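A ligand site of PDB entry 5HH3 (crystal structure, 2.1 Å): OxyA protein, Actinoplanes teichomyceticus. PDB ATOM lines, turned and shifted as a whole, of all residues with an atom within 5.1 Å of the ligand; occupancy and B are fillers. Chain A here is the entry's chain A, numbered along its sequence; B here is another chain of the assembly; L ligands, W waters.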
ATOM      1  N   LEU A  67      10.915   9.733 -37.887  1.00  0.00           N
ATOM      2  CA  LEU A  67      10.969   9.783 -36.418  1.00  0.00           C
ATOM      3  C   LEU A  67      10.355   8.559 -35.741  1.00  0.00           C
ATOM      4  O   LEU A  67      10.660   8.297 -34.590  1.00  0.00           O
ATOM      5  CB  LEU A  67      10.331  11.073 -35.892  1.00  0.00           C
ATOM      6  CG  LEU A  67      11.063  12.378 -36.219  1.00  0.00           C
ATOM      7  CD1 LEU A  67      10.232  13.578 -35.828  1.00  0.00           C
ATOM      8  CD2 LEU A  67      12.423  12.434 -35.528  1.00  0.00           C
ATOM      9  N   LEU A  91      17.807  11.438 -22.411  1.00  0.00           N
ATOM     10  CA  LEU A  91      17.042  10.382 -23.093  1.00  0.00           C
ATOM     11  C   LEU A  91      17.177  10.350 -24.606  1.00  0.00           C
ATOM     12  O   LEU A  91      17.124   9.279 -25.231  1.00  0.00           O
ATOM     13  CB  LEU A  91      15.541  10.489 -22.743  1.00  0.00           C
ATOM     14  CG  LEU A  91      15.208   9.914 -21.359  1.00  0.00           C
ATOM     15  CD1 LEU A  91      13.849  10.391 -20.862  1.00  0.00           C
ATOM     16  CD2 LEU A  91      15.235   8.398 -21.410  1.00  0.00           C
ATOM     17  N   THR A  92      17.363  11.518 -25.207  1.00  0.00           N
ATOM     18  CA  THR A  92      17.379  11.614 -26.651  1.00  0.00           C
ATOM     19  C   THR A  92      18.725  11.080 -27.199  1.00  0.00           C
ATOM     20  O   THR A  92      18.888  10.964 -28.408  1.00  0.00           O
ATOM     21  CB  THR A  92      16.931  13.035 -27.075  1.00  0.00           C
ATOM     22  OG1 THR A  92      16.555  13.066 -28.460  1.00  0.00           O
ATOM     23  CG2 THR A  92      17.981  14.060 -26.771  1.00  0.00           C
ATOM     24  N   HIS A  99      16.728   3.037 -23.717  1.00  0.00           N
ATOM     25  CA  HIS A  99      15.830   4.180 -23.753  1.00  0.00           C
ATOM     26  C   HIS A  99      14.489   3.850 -23.105  1.00  0.00           C
ATOM     27  O   HIS A  99      13.955   4.647 -22.334  1.00  0.00           O
ATOM     28  CB  HIS A  99      15.577   4.615 -25.183  1.00  0.00           C
ATOM     29  CG  HIS A  99      14.561   5.699 -25.297  1.00  0.00           C
ATOM     30  ND1 HIS A  99      13.244   5.446 -25.591  1.00  0.00           N
ATOM     31  CD2 HIS A  99      14.669   7.027 -25.092  1.00  0.00           C
ATOM     32  CE1 HIS A  99      12.585   6.592 -25.597  1.00  0.00           C
ATOM     33  NE2 HIS A  99      13.427   7.563 -25.299  1.00  0.00           N
ATOM     34  N   ARG A 103      12.997   5.833 -19.776  1.00  0.00           N
ATOM     35  CA  ARG A 103      11.805   6.629 -19.991  1.00  0.00           C
ATOM     36  C   ARG A 103      10.592   6.116 -19.190  1.00  0.00           C
ATOM     37  O   ARG A 103       9.824   6.924 -18.679  1.00  0.00           O
ATOM     38  CB  ARG A 103      11.444   6.679 -21.466  1.00  0.00           C
ATOM     39  CG  ARG A 103      10.207   7.499 -21.725  1.00  0.00           C
ATOM     40  CD  ARG A 103      10.229   8.203 -23.046  1.00  0.00           C
ATOM     41  NE  ARG A 103       8.982   8.953 -23.225  1.00  0.00           N
ATOM     42  CZ  ARG A 103       8.801  10.004 -24.014  1.00  0.00           C
ATOM     43  NH1 ARG A 103       9.802  10.493 -24.761  1.00  0.00           N
ATOM     44  NH2 ARG A 103       7.612  10.574 -24.066  1.00  0.00           N
ATOM     45  N   PHE A 110       5.103  12.748 -15.263  1.00  0.00           N
ATOM     46  CA  PHE A 110       4.462  13.581 -16.287  1.00  0.00           C
ATOM     47  C   PHE A 110       3.051  13.126 -16.697  1.00  0.00           C
ATOM     48  O   PHE A 110       2.510  13.621 -17.679  1.00  0.00           O
ATOM     49  CB  PHE A 110       5.388  13.638 -17.508  1.00  0.00           C
ATOM     50  CG  PHE A 110       6.678  14.325 -17.231  1.00  0.00           C
ATOM     51  CD1 PHE A 110       6.788  15.692 -17.378  1.00  0.00           C
ATOM     52  CD2 PHE A 110       7.764  13.599 -16.794  1.00  0.00           C
ATOM     53  CE1 PHE A 110       7.986  16.333 -17.118  1.00  0.00           C
ATOM     54  CE2 PHE A 110       8.959  14.227 -16.514  1.00  0.00           C
ATOM     55  CZ  PHE A 110       9.071  15.608 -16.681  1.00  0.00           C
ATOM     56  N   THR A 155       9.177  25.130 -13.098  1.00  0.00           N
ATOM     57  CA  THR A 155      10.032  23.945 -13.256  1.00  0.00           C
ATOM     58  C   THR A 155      10.686  23.567 -11.915  1.00  0.00           C
ATOM     59  O   THR A 155      10.703  22.387 -11.549  1.00  0.00           O
ATOM     60  CB  THR A 155      11.085  24.181 -14.348  1.00  0.00           C
ATOM     61  OG1 THR A 155      10.405  24.533 -15.560  1.00  0.00           O
ATOM     62  CG2 THR A 155      11.948  22.932 -14.565  1.00  0.00           C
ATOM     63  N   PHE A 234      18.417  17.727 -16.814  1.00  0.00           N
ATOM     64  CA  PHE A 234      17.742  17.873 -18.124  1.00  0.00           C
ATOM     65  C   PHE A 234      16.376  18.595 -18.002  1.00  0.00           C
ATOM     66  O   PHE A 234      16.101  19.538 -18.747  1.00  0.00           O
ATOM     67  CB  PHE A 234      17.559  16.483 -18.745  1.00  0.00           C
ATOM     68  CG  PHE A 234      17.152  16.493 -20.203  1.00  0.00           C
ATOM     69  CD1 PHE A 234      15.882  16.881 -20.591  1.00  0.00           C
ATOM     70  CD2 PHE A 234      18.032  16.045 -21.170  1.00  0.00           C
ATOM     71  CE1 PHE A 234      15.520  16.862 -21.924  1.00  0.00           C
ATOM     72  CE2 PHE A 234      17.655  16.012 -22.505  1.00  0.00           C
ATOM     73  CZ  PHE A 234      16.399  16.413 -22.871  1.00  0.00           C
ATOM     74  N   VAL A 235      15.532  18.142 -17.071  1.00  0.00           N
ATOM     75  CA  VAL A 235      14.212  18.763 -16.874  1.00  0.00           C
ATOM     76  C   VAL A 235      14.328  20.247 -16.500  1.00  0.00           C
ATOM     77  O   VAL A 235      13.582  21.096 -17.021  1.00  0.00           O
ATOM     78  CB  VAL A 235      13.364  17.964 -15.850  1.00  0.00           C
ATOM     79  CG1 VAL A 235      12.113  18.746 -15.448  1.00  0.00           C
ATOM     80  CG2 VAL A 235      12.976  16.635 -16.448  1.00  0.00           C
ATOM     81  N   ALA A 238      15.637  22.040 -19.786  1.00  0.00           N
ATOM     82  CA  ALA A 238      14.534  22.096 -20.768  1.00  0.00           C
ATOM     83  C   ALA A 238      13.457  23.054 -20.294  1.00  0.00           C
ATOM     84  O   ALA A 238      13.044  23.941 -21.040  1.00  0.00           O
ATOM     85  CB  ALA A 238      13.942  20.709 -21.001  1.00  0.00           C
ATOM     86  N   GLY A 239      13.027  22.880 -19.043  1.00  0.00           N
ATOM     87  CA  GLY A 239      12.027  23.757 -18.431  1.00  0.00           C
ATOM     88  C   GLY A 239      12.420  25.209 -18.516  1.00  0.00           C
ATOM     89  O   GLY A 239      11.673  26.015 -19.047  1.00  0.00           O
ATOM     90  N   GLN A 242      13.203  26.023 -22.836  1.00  0.00           N
ATOM     91  CA  GLN A 242      12.046  25.849 -23.740  1.00  0.00           C
ATOM     92  C   GLN A 242      10.843  26.664 -23.295  1.00  0.00           C
ATOM     93  O   GLN A 242      10.256  27.375 -24.103  1.00  0.00           O
ATOM     94  CB  GLN A 242      11.642  24.382 -23.887  1.00  0.00           C
ATOM     95  CG  GLN A 242      12.682  23.495 -24.555  1.00  0.00           C
ATOM     96  CD  GLN A 242      12.746  23.616 -26.067  1.00  0.00           C
ATOM     97  OE1 GLN A 242      12.058  24.425 -26.703  1.00  0.00           O
ATOM     98  NE2 GLN A 242      13.599  22.796 -26.671  1.00  0.00           N
ATOM     99  N   VAL A 243      10.494  26.592 -22.018  1.00  0.00           N
ATOM    100  CA  VAL A 243       9.281  27.252 -21.541  1.00  0.00           C
ATOM    101  C   VAL A 243       9.459  28.773 -21.554  1.00  0.00           C
ATOM    102  O   VAL A 243       8.573  29.487 -22.015  1.00  0.00           O
ATOM    103  CB  VAL A 243       8.851  26.739 -20.145  1.00  0.00           C
ATOM    104  CG1 VAL A 243       7.674  27.547 -19.587  1.00  0.00           C
ATOM    105  CG2 VAL A 243       8.505  25.262 -20.217  1.00  0.00           C
ATOM    106  N   PHE A 246       9.437  30.121 -25.173  1.00  0.00           N
ATOM    107  CA  PHE A 246       8.065  30.053 -25.724  1.00  0.00           C
ATOM    108  C   PHE A 246       7.188  31.171 -25.165  1.00  0.00           C
ATOM    109  O   PHE A 246       6.452  31.820 -25.924  1.00  0.00           O
ATOM    110  CB  PHE A 246       7.412  28.708 -25.430  1.00  0.00           C
ATOM    111  CG  PHE A 246       6.096  28.501 -26.146  1.00  0.00           C
ATOM    112  CD1 PHE A 246       4.906  28.998 -25.616  1.00  0.00           C
ATOM    113  CD2 PHE A 246       6.050  27.794 -27.336  1.00  0.00           C
ATOM    114  CE1 PHE A 246       3.699  28.814 -26.263  1.00  0.00           C
ATOM    115  CE2 PHE A 246       4.842  27.596 -27.983  1.00  0.00           C
ATOM    116  CZ  PHE A 246       3.667  28.107 -27.451  1.00  0.00           C
ATOM    117  N   THR A 284       8.859  26.955 -31.484  1.00  0.00           N
ATOM    118  CA  THR A 284      10.065  27.436 -30.811  1.00  0.00           C
ATOM    119  C   THR A 284      11.188  26.396 -30.678  1.00  0.00           C
ATOM    120  O   THR A 284      12.249  26.720 -30.165  1.00  0.00           O
ATOM    121  CB  THR A 284       9.730  28.058 -29.450  1.00  0.00           C
ATOM    122  OG1 THR A 284       9.122  27.083 -28.605  1.00  0.00           O
ATOM    123  CG2 THR A 284       8.795  29.252 -29.619  1.00  0.00           C
ATOM    124  N   ASP A 285      10.963  25.158 -31.134  1.00  0.00           N
ATOM    125  CA  ASP A 285      12.067  24.228 -31.406  1.00  0.00           C
ATOM    126  C   ASP A 285      11.923  23.815 -32.857  1.00  0.00           C
ATOM    127  O   ASP A 285      11.071  23.006 -33.188  1.00  0.00           O
ATOM    128  CB  ASP A 285      12.051  22.997 -30.480  1.00  0.00           C
ATOM    129  CG  ASP A 285      13.406  22.284 -30.383  1.00  0.00           C
ATOM    130  OD1 ASP A 285      14.396  22.703 -31.030  1.00  0.00           O
ATOM    131  OD2 ASP A 285      13.486  21.286 -29.633  1.00  0.00           O
ATOM    132  N   THR A 288      14.632  18.689 -35.129  1.00  0.00           N
ATOM    133  CA  THR A 288      15.047  17.584 -34.281  1.00  0.00           C
ATOM    134  C   THR A 288      16.543  17.335 -34.489  1.00  0.00           C
ATOM    135  O   THR A 288      17.138  17.772 -35.499  1.00  0.00           O
ATOM    136  CB  THR A 288      14.291  16.282 -34.608  1.00  0.00           C
ATOM    137  OG1 THR A 288      14.491  15.929 -35.983  1.00  0.00           O
ATOM    138  CG2 THR A 288      12.820  16.437 -34.337  1.00  0.00           C
ATOM    139  N   HIS A 289      17.119  16.640 -33.521  1.00  0.00           N
ATOM    140  CA  HIS A 289      18.505  16.172 -33.565  1.00  0.00           C
ATOM    141  C   HIS A 289      18.656  15.172 -34.735  1.00  0.00           C
ATOM    142  O   HIS A 289      17.730  14.376 -34.941  1.00  0.00           O
ATOM    143  CB  HIS A 289      18.838  15.507 -32.216  1.00  0.00           C
ATOM    144  CG  HIS A 289      20.209  14.927 -32.139  1.00  0.00           C
ATOM    145  ND1 HIS A 289      21.346  15.704 -32.197  1.00  0.00           N
ATOM    146  CD2 HIS A 289      20.631  13.646 -32.010  1.00  0.00           C
ATOM    147  CE1 HIS A 289      22.416  14.920 -32.122  1.00  0.00           C
ATOM    148  NE2 HIS A 289      22.016  13.667 -31.999  1.00  0.00           N
ATOM    149  N   ARG A 291      19.134  12.100 -37.110  1.00  0.00           N
ATOM    150  CA  ARG A 291      18.979  10.665 -36.976  1.00  0.00           C
ATOM    151  C   ARG A 291      19.883  10.016 -38.019  1.00  0.00           C
ATOM    152  O   ARG A 291      19.929  10.473 -39.165  1.00  0.00           O
ATOM    153  CB  ARG A 291      17.528  10.228 -37.219  1.00  0.00           C
ATOM    154  CG  ARG A 291      16.455  10.848 -36.309  1.00  0.00           C
ATOM    155  CD  ARG A 291      16.696  10.528 -34.841  1.00  0.00           C
ATOM    156  NE  ARG A 291      15.511  10.665 -33.985  1.00  0.00           N
ATOM    157  CZ  ARG A 291      15.178  11.736 -33.241  1.00  0.00           C
ATOM    158  NH1 ARG A 291      15.922  12.838 -33.224  1.00  0.00           N
ATOM    159  NH2 ARG A 291      14.077  11.684 -32.487  1.00  0.00           N
ATOM    160  N   LEU A 314      10.820  20.725 -38.079  1.00  0.00           N
ATOM    161  CA  LEU A 314       9.531  20.888 -37.422  1.00  0.00           C
ATOM    162  C   LEU A 314       8.873  22.215 -37.841  1.00  0.00           C
ATOM    163  O   LEU A 314       7.643  22.284 -37.971  1.00  0.00           O
ATOM    164  CB  LEU A 314       9.649  20.758 -35.896  1.00  0.00           C
ATOM    165  CG  LEU A 314      10.331  19.488 -35.375  1.00  0.00           C
ATOM    166  CD1 LEU A 314      10.271  19.467 -33.855  1.00  0.00           C
ATOM    167  CD2 LEU A 314       9.722  18.206 -35.931  1.00  0.00           C
ATOM    168  N   ALA A 340       5.429  20.017 -33.198  1.00  0.00           N
ATOM    169  CA  ALA A 340       6.276  20.850 -32.346  1.00  0.00           C
ATOM    170  C   ALA A 340       6.993  20.121 -31.217  1.00  0.00           C
ATOM    171  O   ALA A 340       8.038  20.587 -30.766  1.00  0.00           O
ATOM    172  CB  ALA A 340       5.470  21.993 -31.772  1.00  0.00           C
ATOM    173  N   PHE A 341       6.431  19.006 -30.768  1.00  0.00           N
ATOM    174  CA  PHE A 341       7.051  18.167 -29.745  1.00  0.00           C
ATOM    175  C   PHE A 341       7.606  16.853 -30.318  1.00  0.00           C
ATOM    176  O   PHE A 341       7.817  15.892 -29.567  1.00  0.00           O
ATOM    177  CB  PHE A 341       6.037  17.873 -28.640  1.00  0.00           C
ATOM    178  CG  PHE A 341       5.557  19.106 -27.910  1.00  0.00           C
ATOM    179  CD1 PHE A 341       6.297  19.656 -26.883  1.00  0.00           C
ATOM    180  CD2 PHE A 341       4.327  19.684 -28.236  1.00  0.00           C
ATOM    181  CE1 PHE A 341       5.843  20.775 -26.190  1.00  0.00           C
ATOM    182  CE2 PHE A 341       3.881  20.809 -27.552  1.00  0.00           C
ATOM    183  CZ  PHE A 341       4.629  21.352 -26.535  1.00  0.00           C
ATOM    184  N   GLY A 342       7.865  16.802 -31.611  1.00  0.00           N
ATOM    185  CA  GLY A 342       8.458  15.613 -32.212  1.00  0.00           C
ATOM    186  C   GLY A 342       7.449  14.503 -32.381  1.00  0.00           C
ATOM    187  O   GLY A 342       6.258  14.747 -32.429  1.00  0.00           O
ATOM    188  N   ILE A 345       9.342   7.452 -30.523  1.00  0.00           N
ATOM    189  CA  ILE A 345       9.789   7.120 -29.149  1.00  0.00           C
ATOM    190  C   ILE A 345      10.410   8.283 -28.370  1.00  0.00           C
ATOM    191  O   ILE A 345      10.354   8.295 -27.150  1.00  0.00           O
ATOM    192  CB  ILE A 345      10.730   5.883 -29.089  1.00  0.00           C
ATOM    193  CG1 ILE A 345      12.072   6.156 -29.787  1.00  0.00           C
ATOM    194  CG2 ILE A 345      10.041   4.646 -29.683  1.00  0.00           C
ATOM    195  CD1 ILE A 345      13.134   5.112 -29.519  1.00  0.00           C
ATOM    196  N   HIS A 346      10.999   9.254 -29.075  1.00  0.00           N
ATOM    197  CA  HIS A 346      11.623  10.409 -28.426  1.00  0.00           C
ATOM    198  C   HIS A 346      10.734  11.637 -28.351  1.00  0.00           C
ATOM    199  O   HIS A 346      11.226  12.705 -27.962  1.00  0.00           O
ATOM    200  CB  HIS A 346      12.967  10.767 -29.094  1.00  0.00           C
ATOM    201  CG  HIS A 346      13.991   9.689 -29.000  1.00  0.00           C
ATOM    202  ND1 HIS A 346      14.701   9.427 -27.846  1.00  0.00           N
ATOM    203  CD2 HIS A 346      14.410   8.776 -29.909  1.00  0.00           C
ATOM    204  CE1 HIS A 346      15.511   8.400 -28.050  1.00  0.00           C
ATOM    205  NE2 HIS A 346      15.350   7.988 -29.292  1.00  0.00           N
ATOM    206  N   HIS A 347       9.438  11.524 -28.645  1.00  0.00           N
ATOM    207  CA  HIS A 347       8.528  12.669 -28.531  1.00  0.00           C
ATOM    208  C   HIS A 347       8.554  13.230 -27.100  1.00  0.00           C
ATOM    209  O   HIS A 347       8.670  12.474 -26.109  1.00  0.00           O
ATOM    210  CB  HIS A 347       7.104  12.307 -28.973  1.00  0.00           C
ATOM    211  CG  HIS A 347       6.287  11.620 -27.917  1.00  0.00           C
ATOM    212  ND1 HIS A 347       6.249  10.250 -27.774  1.00  0.00           N
ATOM    213  CD2 HIS A 347       5.508  12.120 -26.932  1.00  0.00           C
ATOM    214  CE1 HIS A 347       5.468   9.929 -26.760  1.00  0.00           C
ATOM    215  NE2 HIS A 347       5.026  11.045 -26.216  1.00  0.00           N
ATOM    216  N   CYS A 348       8.393  14.549 -27.008  1.00  0.00           N
ATOM    217  CA  CYS A 348       8.717  15.306 -25.806  1.00  0.00           C
ATOM    218  C   CYS A 348       8.054  14.733 -24.549  1.00  0.00           C
ATOM    219  O   CYS A 348       6.846  14.803 -24.416  1.00  0.00           O
ATOM    220  CB  CYS A 348       8.321  16.770 -25.955  1.00  0.00           C
ATOM    221  SG  CYS A 348       8.675  17.803 -24.513  1.00  0.00           S
ATOM    222  N   LEU A 349       8.877  14.202 -23.654  1.00  0.00           N
ATOM    223  CA  LEU A 349       8.428  13.745 -22.340  1.00  0.00           C
ATOM    224  C   LEU A 349       7.799  14.867 -21.511  1.00  0.00           C
ATOM    225  O   LEU A 349       6.890  14.615 -20.708  1.00  0.00           O
ATOM    226  CB  LEU A 349       9.590  13.118 -21.557  1.00  0.00           C
ATOM    227  CG  LEU A 349       9.284  12.456 -20.210  1.00  0.00           C
ATOM    228  CD1 LEU A 349       8.414  11.225 -20.417  1.00  0.00           C
ATOM    229  CD2 LEU A 349      10.568  12.084 -19.460  1.00  0.00           C
ATOM    230  N   GLY A 350       8.281  16.094 -21.686  1.00  0.00           N
ATOM    231  CA  GLY A 350       7.773  17.237 -20.928  1.00  0.00           C
ATOM    232  C   GLY A 350       6.562  17.975 -21.475  1.00  0.00           C
ATOM    233  O   GLY A 350       6.176  18.983 -20.916  1.00  0.00           O
ATOM    234  N   ARG A 351       5.987  17.487 -22.579  1.00  0.00           N
ATOM    235  CA  ARG A 351       4.884  18.161 -23.268  1.00  0.00           C
ATOM    236  C   ARG A 351       3.748  18.552 -22.331  1.00  0.00           C
ATOM    237  O   ARG A 351       3.241  19.682 -22.384  1.00  0.00           O
ATOM    238  CB  ARG A 351       4.330  17.297 -24.417  1.00  0.00           C
ATOM    239  CG  ARG A 351       3.234  17.970 -25.205  1.00  0.00           C
ATOM    240  CD  ARG A 351       2.768  17.178 -26.427  1.00  0.00           C
ATOM    241  NE  ARG A 351       1.694  17.908 -27.094  1.00  0.00           N
ATOM    242  CZ  ARG A 351       1.337  17.776 -28.376  1.00  0.00           C
ATOM    243  NH1 ARG A 351       1.949  16.910 -29.189  1.00  0.00           N
ATOM    244  NH2 ARG A 351       0.347  18.517 -28.845  1.00  0.00           N
ATOM    245  N   LEU A 353       3.806  19.103 -19.111  1.00  0.00           N
ATOM    246  CA  LEU A 353       4.219  20.186 -18.197  1.00  0.00           C
ATOM    247  C   LEU A 353       4.297  21.515 -18.939  1.00  0.00           C
ATOM    248  O   LEU A 353       3.833  22.540 -18.446  1.00  0.00           O
ATOM    249  CB  LEU A 353       5.570  19.867 -17.533  1.00  0.00           C
ATOM    250  CG  LEU A 353       6.161  20.898 -16.554  1.00  0.00           C
ATOM    251  CD1 LEU A 353       5.237  21.216 -15.388  1.00  0.00           C
ATOM    252  CD2 LEU A 353       7.499  20.409 -16.019  1.00  0.00           C
ATOM    253  N   ALA A 354       4.890  21.504 -20.125  1.00  0.00           N
ATOM    254  CA  ALA A 354       5.009  22.717 -20.921  1.00  0.00           C
ATOM    255  C   ALA A 354       3.619  23.247 -21.230  1.00  0.00           C
ATOM    256  O   ALA A 354       3.328  24.411 -20.946  1.00  0.00           O
ATOM    257  CB  ALA A 354       5.781  22.456 -22.191  1.00  0.00           C
ATOM    258  N   PHE A 358       1.750  26.811 -20.398  1.00  0.00           N
ATOM    259  CA  PHE A 358       1.263  27.699 -21.460  1.00  0.00           C
ATOM    260  C   PHE A 358      -0.234  27.939 -21.333  1.00  0.00           C
ATOM    261  O   PHE A 358      -0.675  29.080 -21.482  1.00  0.00           O
ATOM    262  CB  PHE A 358       1.578  27.177 -22.864  1.00  0.00           C
ATOM    263  CG  PHE A 358       3.010  26.840 -23.126  1.00  0.00           C
ATOM    264  CD1 PHE A 358       4.059  27.464 -22.446  1.00  0.00           C
ATOM    265  CD2 PHE A 358       3.326  25.896 -24.103  1.00  0.00           C
ATOM    266  CE1 PHE A 358       5.386  27.125 -22.727  1.00  0.00           C
ATOM    267  CE2 PHE A 358       4.631  25.551 -24.385  1.00  0.00           C
ATOM    268  CZ  PHE A 358       5.672  26.169 -23.696  1.00  0.00           C
ATOM    269  N   GLY B   1      12.694  19.527 -24.911  1.00  0.00           N
ATOM    270  CA  GLY B   1      14.105  18.966 -24.881  1.00  0.00           C
ATOM    271  C   GLY B   1      15.377  19.886 -24.839  1.00  0.00           C
ATOM    272  O   GLY B   1      15.321  21.080 -24.626  1.00  0.00           O
HETATM  273  C1  LIG L   1      12.225  15.880 -26.393  1.00  0.00           C
HETATM  274  C2  LIG L   1      11.641  17.302 -21.810  1.00  0.00           C
HETATM  275  C3  LIG L   1       9.603  21.474 -23.326  1.00  0.00           C
HETATM  276  C4  LIG L   1      10.270  20.019 -27.901  1.00  0.00           C
HETATM  277  C5  LIG L   1      12.252  15.938 -25.027  1.00  0.00           C
HETATM  278  C6  LIG L   1      12.766  14.905 -24.211  1.00  0.00           C
HETATM  279  C7  LIG L   1      12.603  15.298 -22.924  1.00  0.00           C
HETATM  280  C8  LIG L   1      11.979  16.568 -22.939  1.00  0.00           C
HETATM  281  C9  LIG L   1      13.039  14.498 -21.706  1.00  0.00           C
HETATM  282  C10 LIG L   1      13.425  13.615 -24.655  1.00  0.00           C
HETATM  283  C11 LIG L   1      12.443  12.447 -24.661  1.00  0.00           C
HETATM  284  C12 LIG L   1      13.107  11.205 -25.205  1.00  0.00           C
HETATM  285  O1  LIG L   1      14.166  11.253 -25.883  1.00  0.00           O
HETATM  286  O2  LIG L   1      12.571  10.094 -24.985  1.00  0.00           O
HETATM  287  C13 LIG L   1      11.030  18.558 -21.814  1.00  0.00           C
HETATM  288  C14 LIG L   1      10.694  19.285 -20.635  1.00  0.00           C
HETATM  289  C15 LIG L   1      10.111  20.466 -21.036  1.00  0.00           C
HETATM  290  C16 LIG L   1      10.110  20.434 -22.521  1.00  0.00           C
HETATM  291  C17 LIG L   1      10.910  18.831 -19.208  1.00  0.00           C
HETATM  292  C18 LIG L   1       9.536  21.591 -20.243  1.00  0.00           C
HETATM  293  C19 LIG L   1       9.375  21.651 -18.922  1.00  0.00           C
HETATM  294  C20 LIG L   1       9.602  21.464 -24.731  1.00  0.00           C
HETATM  295  C21 LIG L   1       9.031  22.443 -25.570  1.00  0.00           C
HETATM  296  C22 LIG L   1       9.223  22.020 -26.884  1.00  0.00           C
HETATM  297  C23 LIG L   1       9.914  20.774 -26.815  1.00  0.00           C
HETATM  298  C24 LIG L   1       8.342  23.721 -25.119  1.00  0.00           C
HETATM  299  C25 LIG L   1       8.813  22.676 -28.159  1.00  0.00           C
HETATM  300  C26 LIG L   1       8.121  23.808 -28.288  1.00  0.00           C
HETATM  301  C27 LIG L   1      10.852  18.772 -27.800  1.00  0.00           C
HETATM  302  C28 LIG L   1      11.175  18.004 -29.019  1.00  0.00           C
HETATM  303  C29 LIG L   1      11.714  16.853 -28.592  1.00  0.00           C
HETATM  304  C30 LIG L   1      11.713  16.934 -27.128  1.00  0.00           C
HETATM  305  C31 LIG L   1      10.985  18.343 -30.493  1.00  0.00           C
HETATM  306  C32 LIG L   1      12.206  15.738 -29.483  1.00  0.00           C
HETATM  307  C33 LIG L   1      13.669  15.958 -29.869  1.00  0.00           C
HETATM  308  C34 LIG L   1      14.118  14.979 -30.935  1.00  0.00           C
HETATM  309  O3  LIG L   1      15.241  15.108 -31.468  1.00  0.00           O
HETATM  310  O4  LIG L   1      13.403  14.021 -31.293  1.00  0.00           O
HETATM  311  N1  LIG L   1      11.749  16.939 -24.246  1.00  0.00           N
HETATM  312  N2  LIG L   1      10.678  19.283 -22.894  1.00  0.00           N
HETATM  313  N3  LIG L   1      10.111  20.455 -25.501  1.00  0.00           N
HETATM  314  N4  LIG L   1      11.196  18.097 -26.681  1.00  0.00           N
HETATM  315 FE1  LIG L   1      10.942  18.654 -24.872  1.00  0.00          FE
HETATM  316  O   HOH W   1      16.678  17.185 -29.861  1.00  0.00           O
HETATM  317  O   HOH W   2      10.654  13.262 -31.416  1.00  0.00           O
HETATM  318  O   HOH W   3      16.150  13.361 -20.750  1.00  0.00           O
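The backbone nitrogen (N) of Gly 1 of chain B binds an iron atom (FE1) of the ligand, 2.0 Å away.
SG of Cys 348 binds FE1 of the ligand (2.4 Å).
NE2 of His 99 lies within hydrogen-bond range of O2 of the ligand (2.7 Å).
NH2 of Arg 291 is in salt-bridge range of O4 of the ligand, at 2.7 Å.
ND1 of His 346 is in hydrogen-bond range of O1 of the ligand (2.7 Å).
NH1 of Arg 103 is in salt-bridge range of O2 of the ligand (2.8 Å).
N of His 289 lies within hydrogen-bond range of O3 of the ligand.
N of Thr 92 sits at hydrogen-bond distance from O1 of the ligand (3.3 Å).
The side-chain amide nitrogen (NE2) of Gln 242 is in hydrogen-bond range of the backbone carbonyl oxygen (O) of Gly 1 of chain B (3.2 Å).
The side-chain sulfur (SG) of Cys 348 lies close to the backbone NH (N) of Gly 350, 3.3 Å away.
SG of Cys 348 lies close to N of Arg 351, 3.3 Å away.
A ring nitrogen (NE2) of His 99 is in hydrogen-bond range of a ring nitrogen (ND1) of His 346 (3.4 Å).
O of His 289 is in hydrogen-bond range of NH1 of Arg 291.
The guanidinium group of Arg 103 sits at hydrogen-bond distance from the backbone carbonyl oxygen of Ile 345 (3.3 Å).
NH1 of Arg 103 is in hydrogen-bond range of O of His 347, at 2.7 Å.
NE2 of Gln 242 sits at hydrogen-bond distance from OD2 of Asp 285, at 3.3 Å.
Residues that only touch the ligand: Leu 91 (3.4 Å), Gly 239 (3.4 Å), Ala 340 (3.4 Å), Phe 234 (3.4 Å), Thr 284 (3.4 Å), Thr 288 (3.5 Å), Ala 238 (3.6 Å), Gly 350 (3.6 Å), Ile 345 (3.6 Å), Gln 242 (3.6 Å), Leu 314 (3.6 Å), Phe 341 (3.7 Å), Gly 342 (3.7 Å), Leu 353 (3.7 Å), Leu 349 (3.7 Å), Val 243 (3.8 Å), Asp 285 (3.9 Å), Phe 358 (3.9 Å) and Val 235 (3.9 Å).
Within 4 Å of the ligand: Leu 91, Thr 92, His 99, Arg 103, Phe 234, Val 235, Ala 238, Gly 239, Gln 242, Val 243, Thr 284, Asp 285, Thr 288, His 289, Arg 291, Leu 314, Ala 340, Phe 341, Gly 342, Ile 345, His 346, Cys 348, Leu 349, Gly 350, Leu 353, Phe 358 and Gly 1 of chain B.
Water W2 lies within hydrogen-bond range of an oxygen (O4) of the ligand (2.9 Å) and the backbone NH (N) of His 347 (3.5 Å).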
